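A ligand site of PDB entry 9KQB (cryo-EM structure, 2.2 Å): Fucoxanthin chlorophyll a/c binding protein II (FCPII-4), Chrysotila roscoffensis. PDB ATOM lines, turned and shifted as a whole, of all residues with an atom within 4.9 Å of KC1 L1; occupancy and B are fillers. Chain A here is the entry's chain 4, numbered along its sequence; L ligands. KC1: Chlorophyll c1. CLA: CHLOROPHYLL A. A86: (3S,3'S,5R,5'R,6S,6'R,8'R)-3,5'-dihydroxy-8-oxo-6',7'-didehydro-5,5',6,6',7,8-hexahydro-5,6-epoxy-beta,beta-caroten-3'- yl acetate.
An oxygen (O1D) of KC1 L1 sits close to the backbone carbonyl oxygen (O) of Gly 104, 3.4 Å away. Val 97 touches KC1 L1 (CG1 to CMA, 3.9 Å). Ala 108 touches KC1 L1. Lys 110 touches KC1 L1. The nearest printed residue that does not touch KC1 L1 is Leu 93 (4.3 Å).
The backbone carbonyl oxygen (O) of Phe 106 is in hydrogen-bond range of the side-chain amino group (NZ) of Lys 110. OD1 of Asp 105 lies within salt-bridge range of NZ of Lys 110 (3.0 Å).
N of Gly 109 sits at hydrogen-bond distance from OBD of KC1 L1 (2.9 Å). The backbone NH of Asp 105 is in hydrogen-bond range of an oxygen (O1D) of KC1 L1, 3.2 Å away. O of Leu 103 is bound to MG of KC1 L1 (2.1 Å). An oxygen (O1D) of KC1 L1 is in hydrogen-bond range of the backbone NH (N) of Phe 106.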
ATOM      1  N   LEU A  93     -19.794 -25.418 -31.092  1.00  0.00           N
ATOM      2  CA  LEU A  93     -18.521 -25.208 -30.403  1.00  0.00           C
ATOM      3  C   LEU A  93     -18.255 -26.341 -29.399  1.00  0.00           C
ATOM      4  O   LEU A  93     -17.116 -26.786 -29.249  1.00  0.00           O
ATOM      5  CB  LEU A  93     -18.517 -23.853 -29.700  1.00  0.00           C
ATOM      6  CG  LEU A  93     -17.178 -23.317 -29.167  1.00  0.00           C
ATOM      7  CD1 LEU A  93     -16.009 -23.729 -30.043  1.00  0.00           C
ATOM      8  CD2 LEU A  93     -17.234 -21.810 -29.008  1.00  0.00           C
ATOM      9  N   VAL A  97     -15.301 -29.605 -29.602  1.00  0.00           N
ATOM     10  CA  VAL A  97     -14.571 -30.184 -28.478  1.00  0.00           C
ATOM     11  C   VAL A  97     -14.958 -31.640 -28.287  1.00  0.00           C
ATOM     12  O   VAL A  97     -14.098 -32.492 -28.018  1.00  0.00           O
ATOM     13  CB  VAL A  97     -14.810 -29.336 -27.215  1.00  0.00           C
ATOM     14  CG1 VAL A  97     -14.693 -30.162 -25.940  1.00  0.00           C
ATOM     15  CG2 VAL A  97     -13.850 -28.152 -27.176  1.00  0.00           C
ATOM     16  N   LEU A 103     -10.604 -27.540 -28.247  1.00  0.00           N
ATOM     17  CA  LEU A 103     -10.123 -26.836 -27.069  1.00  0.00           C
ATOM     18  C   LEU A 103     -10.272 -27.676 -25.803  1.00  0.00           C
ATOM     19  O   LEU A 103     -10.357 -27.121 -24.705  1.00  0.00           O
ATOM     20  CB  LEU A 103     -10.859 -25.497 -26.902  1.00  0.00           C
ATOM     21  CG  LEU A 103     -10.892 -24.573 -28.117  1.00  0.00           C
ATOM     22  CD1 LEU A 103     -12.206 -23.808 -28.160  1.00  0.00           C
ATOM     23  CD2 LEU A 103      -9.713 -23.611 -28.109  1.00  0.00           C
ATOM     24  N   GLY A 104     -10.309 -28.996 -25.946  1.00  0.00           N
ATOM     25  CA  GLY A 104     -10.510 -29.848 -24.791  1.00  0.00           C
ATOM     26  C   GLY A 104      -9.660 -31.096 -24.739  1.00  0.00           C
ATOM     27  O   GLY A 104     -10.053 -32.095 -24.124  1.00  0.00           O
ATOM     28  N   ASP A 105      -8.490 -31.061 -25.369  1.00  0.00           N
ATOM     29  CA  ASP A 105      -7.554 -32.181 -25.307  1.00  0.00           C
ATOM     30  C   ASP A 105      -6.148 -31.595 -25.247  1.00  0.00           C
ATOM     31  O   ASP A 105      -5.519 -31.330 -26.280  1.00  0.00           O
ATOM     32  CB  ASP A 105      -7.717 -33.121 -26.494  1.00  0.00           C
ATOM     33  CG  ASP A 105      -6.845 -34.352 -26.386  1.00  0.00           C
ATOM     34  OD1 ASP A 105      -6.944 -35.061 -25.365  1.00  0.00           O
ATOM     35  OD2 ASP A 105      -6.067 -34.614 -27.325  1.00  0.00           O
ATOM     36  N   PHE A 106      -5.653 -31.398 -24.023  1.00  0.00           N
ATOM     37  CA  PHE A 106      -4.339 -30.807 -23.797  1.00  0.00           C
ATOM     38  C   PHE A 106      -3.619 -31.578 -22.702  1.00  0.00           C
ATOM     39  O   PHE A 106      -4.238 -32.195 -21.837  1.00  0.00           O
ATOM     40  CB  PHE A 106      -4.448 -29.330 -23.423  1.00  0.00           C
ATOM     41  CG  PHE A 106      -5.013 -28.466 -24.505  1.00  0.00           C
ATOM     42  CD1 PHE A 106      -4.235 -28.072 -25.575  1.00  0.00           C
ATOM     43  CD2 PHE A 106      -6.340 -28.054 -24.460  1.00  0.00           C
ATOM     44  CE1 PHE A 106      -4.747 -27.279 -26.582  1.00  0.00           C
ATOM     45  CE2 PHE A 106      -6.864 -27.261 -25.459  1.00  0.00           C
ATOM     46  CZ  PHE A 106      -6.073 -26.871 -26.523  1.00  0.00           C
ATOM     47  N   ALA A 108      -2.000 -30.424 -20.246  1.00  0.00           N
ATOM     48  CA  ALA A 108      -2.116 -29.828 -18.923  1.00  0.00           C
ATOM     49  C   ALA A 108      -3.200 -30.501 -18.102  1.00  0.00           C
ATOM     50  O   ALA A 108      -3.126 -30.518 -16.863  1.00  0.00           O
ATOM     51  CB  ALA A 108      -2.399 -28.329 -19.044  1.00  0.00           C
ATOM     52  N   GLY A 109      -4.213 -31.067 -18.756  1.00  0.00           N
ATOM     53  CA  GLY A 109      -5.264 -31.791 -18.081  1.00  0.00           C
ATOM     54  C   GLY A 109      -5.001 -33.256 -17.855  1.00  0.00           C
ATOM     55  O   GLY A 109      -5.842 -33.946 -17.266  1.00  0.00           O
ATOM     56  N   LYS A 110      -3.859 -33.775 -18.319  1.00  0.00           N
ATOM     57  CA  LYS A 110      -3.492 -35.182 -18.162  1.00  0.00           C
ATOM     58  C   LYS A 110      -2.109 -35.279 -17.538  1.00  0.00           C
ATOM     59  O   LYS A 110      -1.103 -35.420 -18.247  1.00  0.00           O
ATOM     60  CB  LYS A 110      -3.524 -35.921 -19.496  1.00  0.00           C
ATOM     61  CG  LYS A 110      -4.864 -35.853 -20.218  1.00  0.00           C
ATOM     62  CD  LYS A 110      -4.739 -36.368 -21.650  1.00  0.00           C
ATOM     63  CE  LYS A 110      -3.932 -35.408 -22.510  1.00  0.00           C
ATOM     64  NZ  LYS A 110      -4.825 -34.488 -23.287  1.00  0.00           N
HETATM   65  NB  KC1 L   1     -12.607 -25.503 -23.461  1.00  0.00           N
HETATM   66  ND  KC1 L   1      -8.800 -25.979 -22.162  1.00  0.00           N
HETATM   67  C1A KC1 L   1     -10.585 -28.487 -21.322  1.00  0.00           C
HETATM   68  C1B KC1 L   1     -13.654 -26.323 -23.369  1.00  0.00           C
HETATM   69  C1C KC1 L   1     -10.761 -23.135 -24.157  1.00  0.00           C
HETATM   70  C1D KC1 L   1      -7.552 -25.254 -22.212  1.00  0.00           C
HETATM   71  C2A KC1 L   1     -11.328 -29.717 -20.838  1.00  0.00           C
HETATM   72  C2B KC1 L   1     -14.904 -25.843 -24.011  1.00  0.00           C
HETATM   73  C2C KC1 L   1     -10.083 -21.893 -24.599  1.00  0.00           C
HETATM   74  C2D KC1 L   1      -6.399 -25.922 -21.552  1.00  0.00           C
HETATM   75  C3A KC1 L   1     -12.725 -29.466 -21.376  1.00  0.00           C
HETATM   76  C3B KC1 L   1     -14.471 -24.528 -24.557  1.00  0.00           C
HETATM   77  C3C KC1 L   1      -8.696 -22.105 -24.131  1.00  0.00           C
HETATM   78  C3D KC1 L   1      -7.060 -27.170 -21.083  1.00  0.00           C
HETATM   79  C4A KC1 L   1     -12.501 -28.147 -22.053  1.00  0.00           C
HETATM   80  C4B KC1 L   1     -13.044 -24.440 -24.141  1.00  0.00           C
HETATM   81  C4C KC1 L   1      -8.773 -23.438 -23.477  1.00  0.00           C
HETATM   82  C4D KC1 L   1      -8.397 -27.106 -21.461  1.00  0.00           C
HETATM   83  CAA KC1 L   1     -11.502 -29.725 -19.310  1.00  0.00           C
HETATM   84  CAB KC1 L   1     -15.272 -23.544 -25.320  1.00  0.00           C
HETATM   85  CAD KC1 L   1      -6.863 -28.448 -20.350  1.00  0.00           C
HETATM   86  CBB KC1 L   1     -15.401 -22.287 -24.910  1.00  0.00           C
HETATM   87  CBD KC1 L   1      -8.138 -29.190 -20.325  1.00  0.00           C
HETATM   88  CED KC1 L   1      -7.530 -32.904 -21.172  1.00  0.00           C
HETATM   89  CGD KC1 L   1      -7.927 -30.437 -21.116  1.00  0.00           C
HETATM   90  CHA KC1 L   1      -9.120 -28.307 -21.014  1.00  0.00           C
HETATM   91  CHB KC1 L   1     -13.566 -27.610 -22.657  1.00  0.00           C
HETATM   92  CHC KC1 L   1     -12.194 -23.285 -24.473  1.00  0.00           C
HETATM   93  CHD KC1 L   1      -7.513 -23.951 -22.880  1.00  0.00           C
HETATM   94  CMA KC1 L   1     -13.116 -30.555 -22.375  1.00  0.00           C
HETATM   95  CMB KC1 L   1     -16.261 -26.470 -24.106  1.00  0.00           C
HETATM   96  CMD KC1 L   1      -4.943 -25.613 -21.333  1.00  0.00           C
HETATM   97  NA  KC1 L   1     -11.263 -27.628 -21.990  1.00  0.00           N
HETATM   98  NC  KC1 L   1      -9.994 -24.020 -23.506  1.00  0.00           N
HETATM   99  O1D KC1 L   1      -7.772 -30.390 -22.324  1.00  0.00           O
HETATM  100  O2D KC1 L   1      -7.914 -31.736 -20.448  1.00  0.00           O
HETATM  101  OBD KC1 L   1      -5.748 -28.854 -19.852  1.00  0.00           O
HETATM  102 MG   KC1 L   1     -10.664 -25.898 -22.972  1.00  0.00          MG
HETATM  103 MG   CLA L   2     -23.873 -21.347 -16.652  1.00  0.00          MG
HETATM  104  CHA CLA L   2     -25.529 -18.717 -17.712  1.00  0.00           C
HETATM  105  CHB CLA L   2     -26.486 -23.355 -17.005  1.00  0.00           C
HETATM  106  CHC CLA L   2     -21.603 -24.266 -16.966  1.00  0.00           C
HETATM  107  CHD CLA L   2     -21.281 -19.697 -15.120  1.00  0.00           C
HETATM  108  NA  CLA L   2     -25.791 -21.121 -17.370  1.00  0.00           N
HETATM  109  C1A CLA L   2     -26.277 -20.009 -17.764  1.00  0.00           C
HETATM  110  C2A CLA L   2     -27.697 -20.170 -18.237  1.00  0.00           C
HETATM  111  C3A CLA L   2     -28.034 -21.605 -17.873  1.00  0.00           C
HETATM  112  C4A CLA L   2     -26.709 -22.082 -17.387  1.00  0.00           C
HETATM  113  CMA CLA L   2     -29.065 -21.714 -16.769  1.00  0.00           C
HETATM  114  CAA CLA L   2     -27.895 -19.857 -19.729  1.00  0.00           C
HETATM  115  CBA CLA L   2     -27.731 -21.046 -20.671  1.00  0.00           C
HETATM  116  CGA CLA L   2     -26.274 -21.375 -20.837  1.00  0.00           C
HETATM  117  O1A CLA L   2     -25.863 -22.505 -20.651  1.00  0.00           O
HETATM  118  O2A CLA L   2     -25.333 -20.321 -21.200  1.00  0.00           O
HETATM  119  NB  CLA L   2     -24.045 -23.516 -16.873  1.00  0.00           N
HETATM  120  C1B CLA L   2     -25.213 -24.076 -17.227  1.00  0.00           C
HETATM  121  C2B CLA L   2     -25.086 -25.444 -17.777  1.00  0.00           C
HETATM  122  C3B CLA L   2     -23.622 -25.651 -17.735  1.00  0.00           C
HETATM  123  C4B CLA L   2     -23.065 -24.395 -17.165  1.00  0.00           C
HETATM  124  CMB CLA L   2     -26.174 -26.361 -18.260  1.00  0.00           C
HETATM  125  CAB CLA L   2     -22.730 -26.770 -18.125  1.00  0.00           C
HETATM  126  CBB CLA L   2     -22.905 -27.401 -19.279  1.00  0.00           C
HETATM  127  NC  CLA L   2     -21.660 -21.958 -16.194  1.00  0.00           N
HETATM  128  C1C CLA L   2     -21.030 -23.147 -16.170  1.00  0.00           C
HETATM  129  C2C CLA L   2     -19.822 -23.164 -15.320  1.00  0.00           C
HETATM  130  C3C CLA L   2     -19.782 -21.779 -14.794  1.00  0.00           C
HETATM  131  C4C CLA L   2     -20.969 -21.116 -15.403  1.00  0.00           C
HETATM  132  CMC CLA L   2     -18.871 -24.303 -15.058  1.00  0.00           C
HETATM  133  CAC CLA L   2     -18.759 -21.177 -13.866  1.00  0.00           C
HETATM  134  CBC CLA L   2     -17.746 -20.369 -14.656  1.00  0.00           C
HETATM  135  ND  CLA L   2     -23.426 -19.683 -16.305  1.00  0.00           N
HETATM  136  C1D CLA L   2     -22.339 -19.006 -15.894  1.00  0.00           C
HETATM  137  C2D CLA L   2     -22.361 -17.588 -16.302  1.00  0.00           C
HETATM  138  C3D CLA L   2     -23.645 -17.495 -17.033  1.00  0.00           C
HETATM  139  C4D CLA L   2     -24.226 -18.761 -16.997  1.00  0.00           C
HETATM  140  CMD CLA L   2     -21.337 -16.509 -16.045  1.00  0.00           C
HETATM  141  CAD CLA L   2     -24.540 -16.559 -17.777  1.00  0.00           C
HETATM  142  OBD CLA L   2     -24.324 -15.313 -18.004  1.00  0.00           O
HETATM  143  CBD CLA L   2     -25.705 -17.342 -18.250  1.00  0.00           C
HETATM  144  CGD CLA L   2     -26.953 -16.679 -17.759  1.00  0.00           C
HETATM  145  O1D CLA L   2     -27.201 -15.569 -18.220  1.00  0.00           O
HETATM  146  O2D CLA L   2     -27.343 -16.864 -16.374  1.00  0.00           O
HETATM  147  CED CLA L   2     -28.628 -17.409 -16.076  1.00  0.00           C
HETATM  148  C1  CLA L   2     -23.950 -20.585 -21.068  1.00  0.00           C
HETATM  149  C2  CLA L   2     -23.185 -19.293 -21.103  1.00  0.00           C
HETATM  150  C3  CLA L   2     -21.959 -19.219 -20.552  1.00  0.00           C
HETATM  151  C4  CLA L   2     -21.225 -17.911 -20.597  1.00  0.00           C
HETATM  152  C5  CLA L   2     -21.356 -20.442 -19.898  1.00  0.00           C
HETATM  153  C6  CLA L   2     -20.060 -20.110 -19.178  1.00  0.00           C
HETATM  154  C7  CLA L   2     -19.139 -21.312 -19.115  1.00  0.00           C
HETATM  155  C8  CLA L   2     -17.690 -20.818 -19.169  1.00  0.00           C
HETATM  156  C9  CLA L   2     -17.390 -20.176 -20.515  1.00  0.00           C
HETATM  157  C10 CLA L   2     -16.716 -21.947 -18.825  1.00  0.00           C
HETATM  158  C11 CLA L   2     -16.837 -23.183 -19.726  1.00  0.00           C
HETATM  159  C12 CLA L   2     -15.627 -23.354 -20.647  1.00  0.00           C
HETATM  160  C13 CLA L   2     -14.638 -24.443 -20.212  1.00  0.00           C
HETATM  161  C14 CLA L   2     -15.365 -25.736 -19.834  1.00  0.00           C
HETATM  162  C15 CLA L   2     -13.767 -23.944 -19.066  1.00  0.00           C
HETATM  163  C16 CLA L   2     -12.472 -24.742 -18.921  1.00  0.00           C
HETATM  164  C17 CLA L   2     -11.464 -24.324 -19.985  1.00  0.00           C
HETATM  165  C18 CLA L   2     -10.046 -24.245 -19.432  1.00  0.00           C
HETATM  166  C19 CLA L   2      -9.681 -25.462 -18.585  1.00  0.00           C
HETATM  167  C20 CLA L   2      -9.845 -22.945 -18.647  1.00  0.00           C
HETATM  168  NB  KC1 L   3       1.472 -18.484 -24.428  1.00  0.00           N
HETATM  169  ND  KC1 L   3      -0.495 -22.023 -24.666  1.00  0.00           N
HETATM  170  C1A KC1 L   3      -2.453 -19.601 -25.288  1.00  0.00           C
HETATM  171  C1B KC1 L   3       1.075 -17.261 -24.795  1.00  0.00           C
HETATM  172  C1C KC1 L   3       3.233 -20.912 -23.867  1.00  0.00           C
HETATM  173  C1D KC1 L   3      -0.227 -23.418 -24.429  1.00  0.00           C
HETATM  174  C2A KC1 L   3      -3.483 -18.553 -25.616  1.00  0.00           C
HETATM  175  C2B KC1 L   3       2.129 -16.210 -24.766  1.00  0.00           C
HETATM  176  C2C KC1 L   3       4.319 -21.916 -23.976  1.00  0.00           C
HETATM  177  C2D KC1 L   3      -1.406 -24.322 -24.495  1.00  0.00           C
HETATM  178  C3A KC1 L   3      -2.653 -17.286 -25.602  1.00  0.00           C
HETATM  179  C3B KC1 L   3       3.297 -16.992 -24.320  1.00  0.00           C
HETATM  180  C3C KC1 L   3       3.588 -23.197 -24.107  1.00  0.00           C
HETATM  181  C3D KC1 L   3      -2.465 -23.332 -24.808  1.00  0.00           C
HETATM  182  C4A KC1 L   3      -1.319 -17.865 -25.252  1.00  0.00           C
HETATM  183  C4B KC1 L   3       2.768 -18.364 -24.145  1.00  0.00           C
HETATM  184  C4C KC1 L   3       2.172 -22.756 -24.058  1.00  0.00           C
HETATM  185  C4D KC1 L   3      -1.860 -22.077 -24.870  1.00  0.00           C
HETATM  186  CAA KC1 L   3      -4.487 -18.458 -24.472  1.00  0.00           C
HETATM  187  CAB KC1 L   3       4.704 -16.581 -24.087  1.00  0.00           C
HETATM  188  CAC KC1 L   3       4.143 -24.593 -24.253  1.00  0.00           C
HETATM  189  CAD KC1 L   3      -3.918 -23.136 -25.058  1.00  0.00           C
HETATM  190  CBA KC1 L   3      -5.333 -17.192 -24.571  1.00  0.00           C
HETATM  191  CBB KC1 L   3       5.521 -16.412 -25.109  1.00  0.00           C
HETATM  192  CBC KC1 L   3       4.314 -25.122 -22.848  1.00  0.00           C
HETATM  193  CBD KC1 L   3      -4.168 -21.695 -25.299  1.00  0.00           C
HETATM  194  CED KC1 L   3      -6.959 -20.458 -26.814  1.00  0.00           C
HETATM  195  CGA KC1 L   3      -5.185 -16.400 -23.300  1.00  0.00           C
HETATM  196  CGD KC1 L   3      -4.731 -21.550 -26.677  1.00  0.00           C
HETATM  197  CHA KC1 L   3      -2.849 -21.038 -25.187  1.00  0.00           C
HETATM  198  CHB KC1 L   3      -0.317 -16.991 -25.152  1.00  0.00           C
HETATM  199  CHC KC1 L   3       3.598 -19.498 -23.709  1.00  0.00           C
HETATM  200  CHD KC1 L   3       1.153 -23.822 -24.159  1.00  0.00           C
HETATM  201  CMA KC1 L   3      -2.580 -16.694 -26.998  1.00  0.00           C
HETATM  202  CMB KC1 L   3       2.033 -14.739 -25.113  1.00  0.00           C
HETATM  203  CMC KC1 L   3       5.805 -21.685 -23.955  1.00  0.00           C
HETATM  204  CMD KC1 L   3      -1.659 -25.797 -24.343  1.00  0.00           C
HETATM  205  NA  KC1 L   3      -1.267 -19.187 -25.076  1.00  0.00           N
HETATM  206  NC  KC1 L   3       1.981 -21.413 -23.938  1.00  0.00           N
HETATM  207  O1A KC1 L   3      -4.689 -16.903 -22.301  1.00  0.00           O
HETATM  208  O1D KC1 L   3      -4.016 -21.339 -27.640  1.00  0.00           O
HETATM  209  O2A KC1 L   3      -5.630 -15.013 -23.255  1.00  0.00           O
HETATM  210  O2D KC1 L   3      -6.168 -21.640 -26.881  1.00  0.00           O
HETATM  211  OBD KC1 L   3      -4.804 -24.066 -25.082  1.00  0.00           O
HETATM  212 MG   KC1 L   3       0.489 -20.240 -24.730  1.00  0.00          MG
HETATM  213  C   A86 L   4     -19.121 -22.459 -24.335  1.00  0.00           C
HETATM  214  O   A86 L   4     -21.875 -11.158 -28.505  1.00  0.00           O
HETATM  215  C1  A86 L   4     -20.433 -22.151 -23.718  1.00  0.00           C
HETATM  216  C10 A86 L   4     -21.179 -13.431 -27.274  1.00  0.00           C
HETATM  217  C11 A86 L   4     -20.506 -12.271 -27.137  1.00  0.00           C
HETATM  218  C12 A86 L   4     -19.261 -12.187 -26.334  1.00  0.00           C
HETATM  219  C13 A86 L   4     -20.905 -11.113 -27.748  1.00  0.00           C
HETATM  220  C14 A86 L   4     -20.182  -9.802 -27.558  1.00  0.00           C
HETATM  221  C15 A86 L   4     -20.547  -8.588 -28.390  1.00  0.00           C
HETATM  222  C16 A86 L   4     -21.563  -7.613 -27.749  1.00  0.00           C
HETATM  223  C17 A86 L   4     -21.756  -6.314 -28.542  1.00  0.00           C
HETATM  224  C18 A86 L   4     -21.011  -6.203 -29.863  1.00  0.00           C
HETATM  225  C19 A86 L   4     -21.101  -7.514 -30.647  1.00  0.00           C
HETATM  226  C2  A86 L   4     -20.868 -20.811 -23.715  1.00  0.00           C
HETATM  227  C20 A86 L   4     -20.348  -8.537 -29.849  1.00  0.00           C
HETATM  228  C21 A86 L   4     -19.775  -9.679 -30.652  1.00  0.00           C
HETATM  229  C22 A86 L   4     -22.957  -8.246 -27.573  1.00  0.00           C
HETATM  230  C23 A86 L   4     -21.042  -7.192 -26.377  1.00  0.00           C
HETATM  231  C24 A86 L   4     -21.162 -23.223 -23.170  1.00  0.00           C
HETATM  232  C25 A86 L   4     -20.671 -24.455 -22.815  1.00  0.00           C
HETATM  233  C26 A86 L   4     -20.266 -24.894 -21.569  1.00  0.00           C
HETATM  234  C27 A86 L   4     -19.672 -26.109 -21.243  1.00  0.00           C
HETATM  235  C28 A86 L   4     -19.344 -26.403 -19.838  1.00  0.00           C
HETATM  236  C29 A86 L   4     -19.304 -27.130 -22.234  1.00  0.00           C
HETATM  237  C3  A86 L   4     -20.101 -19.681 -23.890  1.00  0.00           C
HETATM  238  C30 A86 L   4     -19.061 -28.374 -21.890  1.00  0.00           C
HETATM  239  C31 A86 L   4     -18.822 -29.582 -21.491  1.00  0.00           C
HETATM  240  C32 A86 L   4     -17.373 -30.112 -21.470  1.00  0.00           C
HETATM  241  C33 A86 L   4     -17.373 -31.616 -21.158  1.00  0.00           C
HETATM  242  C34 A86 L   4     -18.453 -32.443 -21.829  1.00  0.00           C
HETATM  243  C35 A86 L   4     -19.855 -31.850 -21.739  1.00  0.00           C
HETATM  244  C36 A86 L   4     -19.967 -30.496 -21.055  1.00  0.00           C
HETATM  245  C37 A86 L   4     -21.326 -29.886 -21.358  1.00  0.00           C
HETATM  246  C38 A86 L   4     -18.265 -33.844 -23.774  1.00  0.00           C
HETATM  247  C39 A86 L   4     -16.945 -34.539 -23.720  1.00  0.00           C
HETATM  248  C4  A86 L   4     -19.858 -18.907 -25.022  1.00  0.00           C
HETATM  249  C40 A86 L   4     -16.700 -29.862 -22.824  1.00  0.00           C
HETATM  250  C41 A86 L   4     -16.554 -29.375 -20.404  1.00  0.00           C
HETATM  251  C5  A86 L   4     -19.845 -17.537 -25.210  1.00  0.00           C
HETATM  252  C6  A86 L   4     -20.923 -16.641 -25.313  1.00  0.00           C
HETATM  253  C7  A86 L   4     -22.287 -17.155 -25.033  1.00  0.00           C
HETATM  254  C8  A86 L   4     -20.794 -15.286 -25.655  1.00  0.00           C
HETATM  255  C9  A86 L   4     -20.788 -14.710 -26.921  1.00  0.00           C
HETATM  256  O1  A86 L   4     -19.378  -7.932 -28.948  1.00  0.00           O
HETATM  257  O2  A86 L   4     -21.525  -5.127 -30.633  1.00  0.00           O
HETATM  258  O3  A86 L   4     -19.909 -30.747 -19.637  1.00  0.00           O
HETATM  259  O4  A86 L   4     -18.170 -32.601 -23.251  1.00  0.00           O
HETATM  260  O5  A86 L   4     -19.281 -34.287 -24.212  1.00  0.00           O
HETATM  261 MG   CLA L   5     -12.086 -35.629 -13.593  1.00  0.00          MG
HETATM  262  CHA CLA L   5     -13.789 -33.682 -11.780  1.00  0.00           C
HETATM  263  CHB CLA L   5     -12.349 -33.134 -16.253  1.00  0.00           C
HETATM  264  CHC CLA L   5      -9.396 -37.050 -15.561  1.00  0.00           C
HETATM  265  CHD CLA L   5      -8.963 -35.101 -11.085  1.00  0.00           C
HETATM  266  NA  CLA L   5     -13.098 -33.875 -14.120  1.00  0.00           N
HETATM  267  C1A CLA L   5     -13.966 -33.519 -13.262  1.00  0.00           C
HETATM  268  C2A CLA L   5     -15.123 -32.810 -13.933  1.00  0.00           C
HETATM  269  C3A CLA L   5     -14.435 -32.276 -15.190  1.00  0.00           C
HETATM  270  C4A CLA L   5     -13.206 -33.134 -15.220  1.00  0.00           C
HETATM  271  CMA CLA L   5     -15.228 -32.458 -16.473  1.00  0.00           C
HETATM  272  CAA CLA L   5     -15.812 -31.724 -13.104  1.00  0.00           C
HETATM  273  CBA CLA L   5     -15.257 -30.312 -13.247  1.00  0.00           C
HETATM  274  CGA CLA L   5     -14.252 -30.006 -12.157  1.00  0.00           C
HETATM  275  O1A CLA L   5     -14.462 -29.139 -11.330  1.00  0.00           O
HETATM  276  O2A CLA L   5     -13.051 -30.797 -12.088  1.00  0.00           O
HETATM  277  NB  CLA L   5     -10.999 -35.080 -15.636  1.00  0.00           N
HETATM  278  C1B CLA L   5     -11.358 -34.187 -16.570  1.00  0.00           C
HETATM  279  C2B CLA L   5     -10.667 -34.362 -17.871  1.00  0.00           C
HETATM  280  C3B CLA L   5      -9.804 -35.539 -17.609  1.00  0.00           C
HETATM  281  C4B CLA L   5     -10.100 -35.921 -16.201  1.00  0.00           C
HETATM  282  CMB CLA L   5     -10.805 -33.557 -19.137  1.00  0.00           C
HETATM  283  CAB CLA L   5      -8.832 -36.312 -18.415  1.00  0.00           C
HETATM  284  CBB CLA L   5      -9.248 -37.299 -19.188  1.00  0.00           C
HETATM  285  NC  CLA L   5      -9.424 -36.042 -13.383  1.00  0.00           N
HETATM  286  C1C CLA L   5      -8.707 -36.693 -14.301  1.00  0.00           C
HETATM  287  C2C CLA L   5      -7.304 -36.961 -13.914  1.00  0.00           C
HETATM  288  C3C CLA L   5      -7.237 -36.346 -12.563  1.00  0.00           C
HETATM  289  C4C CLA L   5      -8.610 -35.796 -12.340  1.00  0.00           C
HETATM  290  CMC CLA L   5      -6.217 -37.656 -14.687  1.00  0.00           C
HETATM  291  CAC CLA L   5      -6.052 -36.286 -11.633  1.00  0.00           C
HETATM  292  CBC CLA L   5      -5.388 -34.932 -11.759  1.00  0.00           C
HETATM  293  ND  CLA L   5     -11.168 -34.419 -11.890  1.00  0.00           N
HETATM  294  C1D CLA L   5     -10.367 -34.705 -10.851  1.00  0.00           C
HETATM  295  C2D CLA L   5     -11.055 -34.567  -9.552  1.00  0.00           C
HETATM  296  C3D CLA L   5     -12.415 -34.146  -9.958  1.00  0.00           C
HETATM  297  C4D CLA L   5     -12.420 -34.075 -11.353  1.00  0.00           C
HETATM  298  CMD CLA L   5     -10.507 -34.795  -8.174  1.00  0.00           C
HETATM  299  CAD CLA L   5     -13.780 -33.779  -9.462  1.00  0.00           C
HETATM  300  OBD CLA L   5     -14.159 -33.728  -8.241  1.00  0.00           O
HETATM  301  CBD CLA L   5     -14.646 -34.034 -10.630  1.00  0.00           C
HETATM  302  CGD CLA L   5     -15.012 -35.490 -10.696  1.00  0.00           C
HETATM  303  O1D CLA L   5     -15.834 -35.816 -11.541  1.00  0.00           O
HETATM  304  O2D CLA L   5     -14.986 -36.283  -9.482  1.00  0.00           O
HETATM  305  CED CLA L   5     -13.932 -37.214  -9.197  1.00  0.00           C
HETATM  306  C1  CLA L   5     -11.741 -30.246 -12.151  1.00  0.00           C
HETATM  307  C2  CLA L   5     -10.926 -31.248 -12.932  1.00  0.00           C
HETATM  308  C3  CLA L   5      -9.590 -31.329 -12.867  1.00  0.00           C
HETATM  309  C4  CLA L   5      -8.808 -30.403 -11.990  1.00  0.00           C
HETATM  310  C5  CLA L   5      -8.876 -32.377 -13.701  1.00  0.00           C
HETATM  311  C6  CLA L   5      -7.844 -31.713 -14.596  1.00  0.00           C
HETATM  312  C7  CLA L   5      -8.489 -30.931 -15.734  1.00  0.00           C
HETATM  313  C8  CLA L   5      -8.324 -29.423 -15.567  1.00  0.00           C
HETATM  314  C9  CLA L   5      -9.535 -28.685 -16.133  1.00  0.00           C
HETATM  315  C10 CLA L   5      -7.034 -28.958 -16.224  1.00  0.00           C
HETATM  316  C11 CLA L   5      -5.960 -28.644 -15.186  1.00  0.00           C
